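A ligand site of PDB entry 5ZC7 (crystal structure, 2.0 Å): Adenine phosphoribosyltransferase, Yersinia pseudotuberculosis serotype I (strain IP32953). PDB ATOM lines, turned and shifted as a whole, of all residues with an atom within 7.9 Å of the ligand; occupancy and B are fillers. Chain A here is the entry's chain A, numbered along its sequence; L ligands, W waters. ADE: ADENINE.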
ATOM      1  N   LYS A  20      -7.230  33.794 -22.878  1.00  0.00           N
ATOM      2  CA  LYS A  20      -8.337  33.011 -23.434  1.00  0.00           C
ATOM      3  C   LYS A  20      -8.027  31.560 -23.424  1.00  0.00           C
ATOM      4  O   LYS A  20      -6.851  31.169 -23.594  1.00  0.00           O
ATOM      5  CB  LYS A  20      -8.597  33.421 -24.859  1.00  0.00           C
ATOM      6  CG  LYS A  20      -9.399  34.751 -24.892  1.00  0.00           C
ATOM      7  CD  LYS A  20      -9.648  34.897 -26.367  1.00  0.00           C
ATOM      8  CE  LYS A  20      -9.685  36.302 -26.841  1.00  0.00           C
ATOM      9  NZ  LYS A  20     -10.826  36.868 -26.161  1.00  0.00           N
ATOM     10  N   THR A  21      -9.060  30.762 -23.218  1.00  0.00           N
ATOM     11  CA  THR A  21      -9.026  29.341 -23.418  1.00  0.00           C
ATOM     12  C   THR A  21      -9.554  28.931 -24.729  1.00  0.00           C
ATOM     13  O   THR A  21     -10.704  29.170 -25.071  1.00  0.00           O
ATOM     14  CB  THR A  21      -9.665  28.548 -22.256  1.00  0.00           C
ATOM     15  OG1 THR A  21      -8.916  28.793 -21.069  1.00  0.00           O
ATOM     16  CG2 THR A  21      -9.535  27.107 -22.533  1.00  0.00           C
ATOM     17  N   ILE A  22      -8.745  28.159 -25.459  1.00  0.00           N
ATOM     18  CA  ILE A  22      -9.110  27.756 -26.828  1.00  0.00           C
ATOM     19  C   ILE A  22      -9.222  26.233 -26.890  1.00  0.00           C
ATOM     20  O   ILE A  22      -8.199  25.542 -26.955  1.00  0.00           O
ATOM     21  CB  ILE A  22      -8.125  28.246 -27.902  1.00  0.00           C
ATOM     22  CG1 ILE A  22      -7.834  29.741 -27.743  1.00  0.00           C
ATOM     23  CG2 ILE A  22      -8.684  27.963 -29.315  1.00  0.00           C
ATOM     24  CD1 ILE A  22      -9.044  30.652 -27.865  1.00  0.00           C
ATOM     25  N   TYR A  25      -7.120  23.004 -29.514  1.00  0.00           N
ATOM     26  CA  TYR A  25      -5.842  23.317 -30.022  1.00  0.00           C
ATOM     27  C   TYR A  25      -4.690  22.836 -29.075  1.00  0.00           C
ATOM     28  O   TYR A  25      -4.755  23.073 -27.890  1.00  0.00           O
ATOM     29  CB  TYR A  25      -5.770  24.792 -30.379  1.00  0.00           C
ATOM     30  CG  TYR A  25      -4.475  25.164 -31.009  1.00  0.00           C
ATOM     31  CD1 TYR A  25      -3.377  25.436 -30.237  1.00  0.00           C
ATOM     32  CD2 TYR A  25      -4.340  25.203 -32.418  1.00  0.00           C
ATOM     33  CE1 TYR A  25      -2.192  25.715 -30.783  1.00  0.00           C
ATOM     34  CE2 TYR A  25      -3.112  25.521 -32.971  1.00  0.00           C
ATOM     35  CZ  TYR A  25      -2.074  25.802 -32.190  1.00  0.00           C
ATOM     36  OH  TYR A  25      -0.855  26.124 -32.689  1.00  0.00           O
ATOM     37  N   PRO A  26      -3.646  22.166 -29.581  1.00  0.00           N
ATOM     38  CA  PRO A  26      -3.420  21.841 -31.010  1.00  0.00           C
ATOM     39  C   PRO A  26      -4.118  20.579 -31.462  1.00  0.00           C
ATOM     40  O   PRO A  26      -4.038  20.247 -32.629  1.00  0.00           O
ATOM     41  CB  PRO A  26      -1.901  21.567 -31.089  1.00  0.00           C
ATOM     42  CG  PRO A  26      -1.429  21.289 -29.679  1.00  0.00           C
ATOM     43  CD  PRO A  26      -2.473  21.898 -28.722  1.00  0.00           C
ATOM     44  N   GLY A  29      -9.338  17.728 -27.160  1.00  0.00           N
ATOM     45  CA  GLY A  29      -9.338  17.607 -25.744  1.00  0.00           C
ATOM     46  C   GLY A  29      -8.428  18.552 -25.036  1.00  0.00           C
ATOM     47  O   GLY A  29      -8.552  18.634 -23.838  1.00  0.00           O
ATOM     48  N   ILE A  30      -7.496  19.232 -25.690  1.00  0.00           N
ATOM     49  CA  ILE A  30      -6.605  20.134 -24.949  1.00  0.00           C
ATOM     50  C   ILE A  30      -7.339  21.473 -24.812  1.00  0.00           C
ATOM     51  O   ILE A  30      -7.945  21.947 -25.792  1.00  0.00           O
ATOM     52  CB  ILE A  30      -5.264  20.382 -25.695  1.00  0.00           C
ATOM     53  CG1 ILE A  30      -4.405  19.096 -25.834  1.00  0.00           C
ATOM     54  CG2 ILE A  30      -4.467  21.459 -25.017  1.00  0.00           C
ATOM     55  CD1 ILE A  30      -4.422  18.157 -24.630  1.00  0.00           C
ATOM     56  N   LEU A  31      -7.284  22.091 -23.648  1.00  0.00           N
ATOM     57  CA  LEU A  31      -7.876  23.412 -23.397  1.00  0.00           C
ATOM     58  C   LEU A  31      -6.710  24.375 -23.467  1.00  0.00           C
ATOM     59  O   LEU A  31      -5.974  24.566 -22.487  1.00  0.00           O
ATOM     60  CB  LEU A  31      -8.566  23.495 -22.032  1.00  0.00           C
ATOM     61  CG  LEU A  31      -9.806  22.620 -21.944  1.00  0.00           C
ATOM     62  CD1 LEU A  31     -10.359  22.519 -20.553  1.00  0.00           C
ATOM     63  CD2 LEU A  31     -10.899  23.011 -22.928  1.00  0.00           C
ATOM     64  N   PHE A  32      -6.434  24.913 -24.646  1.00  0.00           N
ATOM     65  CA  PHE A  32      -5.210  25.660 -24.823  1.00  0.00           C
ATOM     66  C   PHE A  32      -5.301  27.022 -24.135  1.00  0.00           C
ATOM     67  O   PHE A  32      -6.303  27.780 -24.305  1.00  0.00           O
ATOM     68  CB  PHE A  32      -4.930  25.866 -26.314  1.00  0.00           C
ATOM     69  CG  PHE A  32      -3.558  26.359 -26.637  1.00  0.00           C
ATOM     70  CD1 PHE A  32      -2.468  25.420 -26.652  1.00  0.00           C
ATOM     71  CD2 PHE A  32      -3.326  27.699 -26.867  1.00  0.00           C
ATOM     72  CE1 PHE A  32      -1.163  25.856 -26.887  1.00  0.00           C
ATOM     73  CE2 PHE A  32      -2.029  28.169 -27.094  1.00  0.00           C
ATOM     74  CZ  PHE A  32      -0.969  27.243 -27.123  1.00  0.00           C
ATOM     75  N   ARG A  33      -4.259  27.343 -23.407  1.00  0.00           N
ATOM     76  CA  ARG A  33      -4.165  28.650 -22.722  1.00  0.00           C
ATOM     77  C   ARG A  33      -3.401  29.625 -23.590  1.00  0.00           C
ATOM     78  O   ARG A  33      -2.194  29.410 -23.785  1.00  0.00           O
ATOM     79  CB  ARG A  33      -3.543  28.515 -21.327  1.00  0.00           C
ATOM     80  CG  ARG A  33      -3.984  27.315 -20.568  1.00  0.00           C
ATOM     81  CD  ARG A  33      -5.492  27.260 -20.254  1.00  0.00           C
ATOM     82  NE  ARG A  33      -5.906  26.052 -19.562  1.00  0.00           N
ATOM     83  CZ  ARG A  33      -7.173  25.747 -19.239  1.00  0.00           C
ATOM     84  NH1 ARG A  33      -7.424  24.608 -18.652  1.00  0.00           N
ATOM     85  NH2 ARG A  33      -8.205  26.565 -19.495  1.00  0.00           N
ATOM     86  N   ASP A  34      -4.104  30.588 -24.170  1.00  0.00           N
ATOM     87  CA  ASP A  34      -3.606  31.511 -25.174  1.00  0.00           C
ATOM     88  C   ASP A  34      -3.150  32.816 -24.602  1.00  0.00           C
ATOM     89  O   ASP A  34      -3.916  33.738 -24.421  1.00  0.00           O
ATOM     90  CB  ASP A  34      -4.692  31.777 -26.135  1.00  0.00           C
ATOM     91  CG  ASP A  34      -4.277  32.705 -27.304  1.00  0.00           C
ATOM     92  OD1 ASP A  34      -3.079  32.944 -27.541  1.00  0.00           O
ATOM     93  OD2 ASP A  34      -5.237  33.085 -28.017  1.00  0.00           O
ATOM     94  N   VAL A  35      -1.831  32.938 -24.445  1.00  0.00           N
ATOM     95  CA  VAL A  35      -1.255  34.111 -23.917  1.00  0.00           C
ATOM     96  C   VAL A  35      -1.346  35.352 -24.854  1.00  0.00           C
ATOM     97  O   VAL A  35      -1.185  36.504 -24.397  1.00  0.00           O
ATOM     98  CB  VAL A  35       0.172  33.790 -23.439  1.00  0.00           C
ATOM     99  CG1 VAL A  35       1.179  33.818 -24.558  1.00  0.00           C
ATOM    100  CG2 VAL A  35       0.492  34.752 -22.372  1.00  0.00           C
ATOM    101  N   ARG A  70       8.116  32.903 -27.344  1.00  0.00           N
ATOM    102  CA  ARG A  70       7.162  33.568 -26.457  1.00  0.00           C
ATOM    103  C   ARG A  70       7.829  34.031 -25.181  1.00  0.00           C
ATOM    104  O   ARG A  70       7.469  35.075 -24.637  1.00  0.00           O
ATOM    105  CB  ARG A  70       5.833  32.795 -26.223  1.00  0.00           C
ATOM    106  CG  ARG A  70       4.862  32.858 -27.418  1.00  0.00           C
ATOM    107  CD  ARG A  70       3.455  32.210 -27.188  1.00  0.00           C
ATOM    108  NE  ARG A  70       3.704  30.855 -26.696  1.00  0.00           N
ATOM    109  CZ  ARG A  70       3.331  29.716 -27.281  1.00  0.00           C
ATOM    110  NH1 ARG A  70       2.560  29.676 -28.368  1.00  0.00           N
ATOM    111  NH2 ARG A  70       3.724  28.579 -26.736  1.00  0.00           N
ATOM    112  N   ASP A 131       6.825  32.139 -20.790  1.00  0.00           N
ATOM    113  CA  ASP A 131       5.413  32.433 -20.801  1.00  0.00           C
ATOM    114  C   ASP A 131       4.657  31.410 -19.976  1.00  0.00           C
ATOM    115  O   ASP A 131       3.816  31.814 -19.182  1.00  0.00           O
ATOM    116  CB  ASP A 131       4.799  32.601 -22.210  1.00  0.00           C
ATOM    117  CG  ASP A 131       4.940  31.455 -23.061  1.00  0.00           C
ATOM    118  OD1 ASP A 131       5.897  30.726 -22.900  1.00  0.00           O
ATOM    119  OD2 ASP A 131       4.103  31.342 -23.971  1.00  0.00           O
ATOM    120  N   LEU A 132       4.975  30.150 -20.141  1.00  0.00           N
ATOM    121  CA  LEU A 132       4.049  29.084 -19.750  1.00  0.00           C
ATOM    122  C   LEU A 132       4.876  27.867 -19.323  1.00  0.00           C
ATOM    123  O   LEU A 132       5.722  27.388 -20.074  1.00  0.00           O
ATOM    124  CB  LEU A 132       3.066  28.722 -20.896  1.00  0.00           C
ATOM    125  CG  LEU A 132       2.023  27.687 -20.443  1.00  0.00           C
ATOM    126  CD1 LEU A 132       0.641  27.868 -21.071  1.00  0.00           C
ATOM    127  CD2 LEU A 132       2.416  26.225 -20.652  1.00  0.00           C
ATOM    128  N   LEU A 133       4.619  27.353 -18.141  1.00  0.00           N
ATOM    129  CA  LEU A 133       5.335  26.138 -17.681  1.00  0.00           C
ATOM    130  C   LEU A 133       4.415  24.977 -17.838  1.00  0.00           C
ATOM    131  O   LEU A 133       3.375  24.869 -17.157  1.00  0.00           O
ATOM    132  CB  LEU A 133       5.786  26.285 -16.204  1.00  0.00           C
ATOM    133  CG  LEU A 133       6.529  25.063 -15.645  1.00  0.00           C
ATOM    134  CD1 LEU A 133       7.794  24.726 -16.462  1.00  0.00           C
ATOM    135  CD2 LEU A 133       6.835  25.413 -14.157  1.00  0.00           C
ATOM    136  N   ALA A 134       4.816  24.040 -18.692  1.00  0.00           N
ATOM    137  CA  ALA A 134       4.033  22.841 -18.966  1.00  0.00           C
ATOM    138  C   ALA A 134       4.874  21.690 -18.403  1.00  0.00           C
ATOM    139  O   ALA A 134       4.904  21.429 -17.217  1.00  0.00           O
ATOM    140  CB  ALA A 134       3.770  22.693 -20.517  1.00  0.00           C
ATOM    141  N   THR A 135       5.548  20.936 -19.257  1.00  0.00           N
ATOM    142  CA  THR A 135       6.354  19.794 -18.729  1.00  0.00           C
ATOM    143  C   THR A 135       7.763  20.231 -18.233  1.00  0.00           C
ATOM    144  O   THR A 135       8.457  19.479 -17.553  1.00  0.00           O
ATOM    145  CB  THR A 135       6.577  18.673 -19.811  1.00  0.00           C
ATOM    146  OG1 THR A 135       7.375  19.208 -20.822  1.00  0.00           O
ATOM    147  CG2 THR A 135       5.347  18.127 -20.361  1.00  0.00           C
ATOM    148  N   ILE A 160       2.115  31.717 -16.794  1.00  0.00           N
ATOM    149  CA  ILE A 160       1.212  30.651 -16.622  1.00  0.00           C
ATOM    150  C   ILE A 160       1.888  29.370 -16.203  1.00  0.00           C
ATOM    151  O   ILE A 160       2.892  28.975 -16.776  1.00  0.00           O
ATOM    152  CB  ILE A 160       0.446  30.405 -17.951  1.00  0.00           C
ATOM    153  CG1 ILE A 160      -0.248  31.690 -18.419  1.00  0.00           C
ATOM    154  CG2 ILE A 160      -0.554  29.298 -17.716  1.00  0.00           C
ATOM    155  CD1 ILE A 160      -0.710  31.644 -19.841  1.00  0.00           C
ATOM    156  N   LEU A 162       0.939  25.190 -15.602  1.00  0.00           N
ATOM    157  CA  LEU A 162       0.111  24.034 -15.675  1.00  0.00           C
ATOM    158  C   LEU A 162       0.683  22.937 -14.760  1.00  0.00           C
ATOM    159  O   LEU A 162       1.398  22.038 -15.198  1.00  0.00           O
ATOM    160  CB  LEU A 162      -0.028  23.555 -17.077  1.00  0.00           C
ATOM    161  CG  LEU A 162      -0.451  24.685 -18.053  1.00  0.00           C
ATOM    162  CD1 LEU A 162      -0.559  24.110 -19.460  1.00  0.00           C
ATOM    163  CD2 LEU A 162      -1.723  25.449 -17.727  1.00  0.00           C
ATOM    164  N   LEU A 165       1.100  19.143 -15.413  1.00  0.00           N
ATOM    165  CA  LEU A 165       2.050  18.565 -16.352  1.00  0.00           C
ATOM    166  C   LEU A 165       3.428  18.279 -15.737  1.00  0.00           C
ATOM    167  O   LEU A 165       4.298  17.880 -16.503  1.00  0.00           O
ATOM    168  CB  LEU A 165       2.203  19.402 -17.625  1.00  0.00           C
ATOM    169  CG  LEU A 165       0.959  19.331 -18.500  1.00  0.00           C
ATOM    170  CD1 LEU A 165       0.999  20.384 -19.608  1.00  0.00           C
ATOM    171  CD2 LEU A 165       0.829  17.873 -19.112  1.00  0.00           C
ATOM    172  N   PHE A 184      -3.583  27.082 -14.231  1.00  0.00           N
ATOM    173  CA  PHE A 184      -4.765  26.437 -14.747  1.00  0.00           C
ATOM    174  C   PHE A 184      -4.602  24.982 -14.484  1.00  0.00           C
ATOM    175  O   PHE A 184      -3.459  24.465 -14.555  1.00  0.00           O
ATOM    176  CB  PHE A 184      -4.936  26.633 -16.292  1.00  0.00           C
ATOM    177  CG  PHE A 184      -5.130  28.053 -16.714  1.00  0.00           C
ATOM    178  CD1 PHE A 184      -6.367  28.617 -16.715  1.00  0.00           C
ATOM    179  CD2 PHE A 184      -4.031  28.861 -17.100  1.00  0.00           C
ATOM    180  CE1 PHE A 184      -6.544  29.940 -17.171  1.00  0.00           C
ATOM    181  CE2 PHE A 184      -4.210  30.155 -17.511  1.00  0.00           C
ATOM    182  CZ  PHE A 184      -5.496  30.723 -17.557  1.00  0.00           C
ATOM    183  N   ASP A 185      -5.728  24.276 -14.248  1.00  0.00           N
ATOM    184  CA  ASP A 185      -5.729  22.800 -14.198  1.00  0.00           C
ATOM    185  C   ASP A 185      -5.661  22.236 -15.601  1.00  0.00           C
ATOM    186  O   ASP A 185      -5.780  22.921 -16.630  1.00  0.00           O
ATOM    187  CB  ASP A 185      -6.990  22.309 -13.516  1.00  0.00           C
ATOM    188  CG  ASP A 185      -7.223  23.033 -12.192  1.00  0.00           C
ATOM    189  OD1 ASP A 185      -6.260  22.873 -11.389  1.00  0.00           O
ATOM    190  OD2 ASP A 185      -8.259  23.847 -12.129  1.00  0.00           O
ATOM    191  N   GLY A 186      -5.488  20.950 -15.631  1.00  0.00           N
ATOM    192  CA  GLY A 186      -5.558  20.267 -16.880  1.00  0.00           C
ATOM    193  C   GLY A 186      -4.257  20.194 -17.622  1.00  0.00           C
ATOM    194  O   GLY A 186      -3.224  20.739 -17.214  1.00  0.00           O
ATOM    195  N   HIS A 187      -4.341  19.554 -18.787  1.00  0.00           N
ATOM    196  CA  HIS A 187      -3.149  19.221 -19.544  1.00  0.00           C
ATOM    197  C   HIS A 187      -2.896  20.274 -20.656  1.00  0.00           C
ATOM    198  O   HIS A 187      -3.573  21.334 -20.753  1.00  0.00           O
ATOM    199  CB  HIS A 187      -3.263  17.748 -20.048  1.00  0.00           C
ATOM    200  CG  HIS A 187      -3.035  16.712 -18.966  1.00  0.00           C
ATOM    201  ND1 HIS A 187      -2.751  15.376 -19.237  1.00  0.00           N
ATOM    202  CD2 HIS A 187      -3.001  16.828 -17.614  1.00  0.00           C
ATOM    203  CE1 HIS A 187      -2.547  14.726 -18.097  1.00  0.00           C
ATOM    204  NE2 HIS A 187      -2.668  15.590 -17.105  1.00  0.00           N
ATOM    205  OXT HIS A 187      -1.953  20.160 -21.469  1.00  0.00           O
HETATM  206  N9  ADE L   1       1.237  23.215 -23.268  1.00  0.00           N
HETATM  207  C8  ADE L   1       0.752  22.039 -22.786  1.00  0.00           C
HETATM  208  N7  ADE L   1      -0.568  22.211 -22.546  1.00  0.00           N
HETATM  209  C5  ADE L   1      -0.890  23.446 -22.882  1.00  0.00           C
HETATM  210  C6  ADE L   1      -2.130  24.193 -22.759  1.00  0.00           C
HETATM  211  N6  ADE L   1      -3.249  23.651 -22.259  1.00  0.00           N
HETATM  212  N1  ADE L   1      -2.101  25.448 -23.130  1.00  0.00           N
HETATM  213  C2  ADE L   1      -0.958  26.054 -23.556  1.00  0.00           C
HETATM  214  N3  ADE L   1       0.213  25.383 -23.726  1.00  0.00           N
HETATM  215  C4  ADE L   1       0.274  24.104 -23.340  1.00  0.00           C
HETATM  216  O   HOH W   1       2.358  26.834 -24.550  1.00  0.00           O
HETATM  217  O   HOH W   2      -4.453  23.541 -19.074  1.00  0.00           O
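Merely in contact with the ligand: Phe 32 (3.3 Å), Leu 132 (3.5 Å), Leu 162 (3.5 Å), Leu 165 (3.6 Å), Ile 30 (3.7 Å) and Ala 134 (3.8 Å). Hydrophobic or aromatic side chains within 4 Å of the ligand: Ile 30, Phe 32, Leu 132, Ala 134, Leu 162 and Leu 165. Within 4 Å of the ligand: Ile 30, Leu 31, Phe 32, Arg 33, Leu 132, Ala 134, Leu 162, Leu 165 and His 187.
O of Asp 185 is in hydrogen-bond range of NH1 of Arg 33, 3.1 Å away. The side-chain hydroxyl (OG1) of Thr 21 is in hydrogen-bond range of the guanidinium group (NH2) of Arg 33 (2.8 Å). The backbone carbonyl oxygen (O) of Leu 31 lies within hydrogen-bond range of the guanidinium group (NE) of Arg 33, at 3.3 Å. N of Ile 22 is in hydrogen-bond range of O of Phe 32 (2.7 Å). The backbone carbonyl oxygen of Leu 133 is in hydrogen-bond range of the backbone NH of Leu 162 (2.9 Å).
Water W1 lies within hydrogen-bond range of N3 of the ligand (2.7 Å) and NH2 of Arg 70 (3.1 Å). Water W2 lies within hydrogen-bond range of O of Asp 185 (2.8 Å), O of His 187 (2.9 Å), NE of Arg 33 (2.9 Å) and N6 of the ligand (3.4 Å).
The chain-end carboxylate (OXT) of His 187 sits at hydrogen-bond distance from a nitrogen (N7) of the ligand. A nitrogen (N1) of the ligand sits at hydrogen-bond distance from the backbone NH (N) of Arg 33 (2.9 Å). O of Leu 31 lies within hydrogen-bond range of N6 of the ligand, at 2.9 Å.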
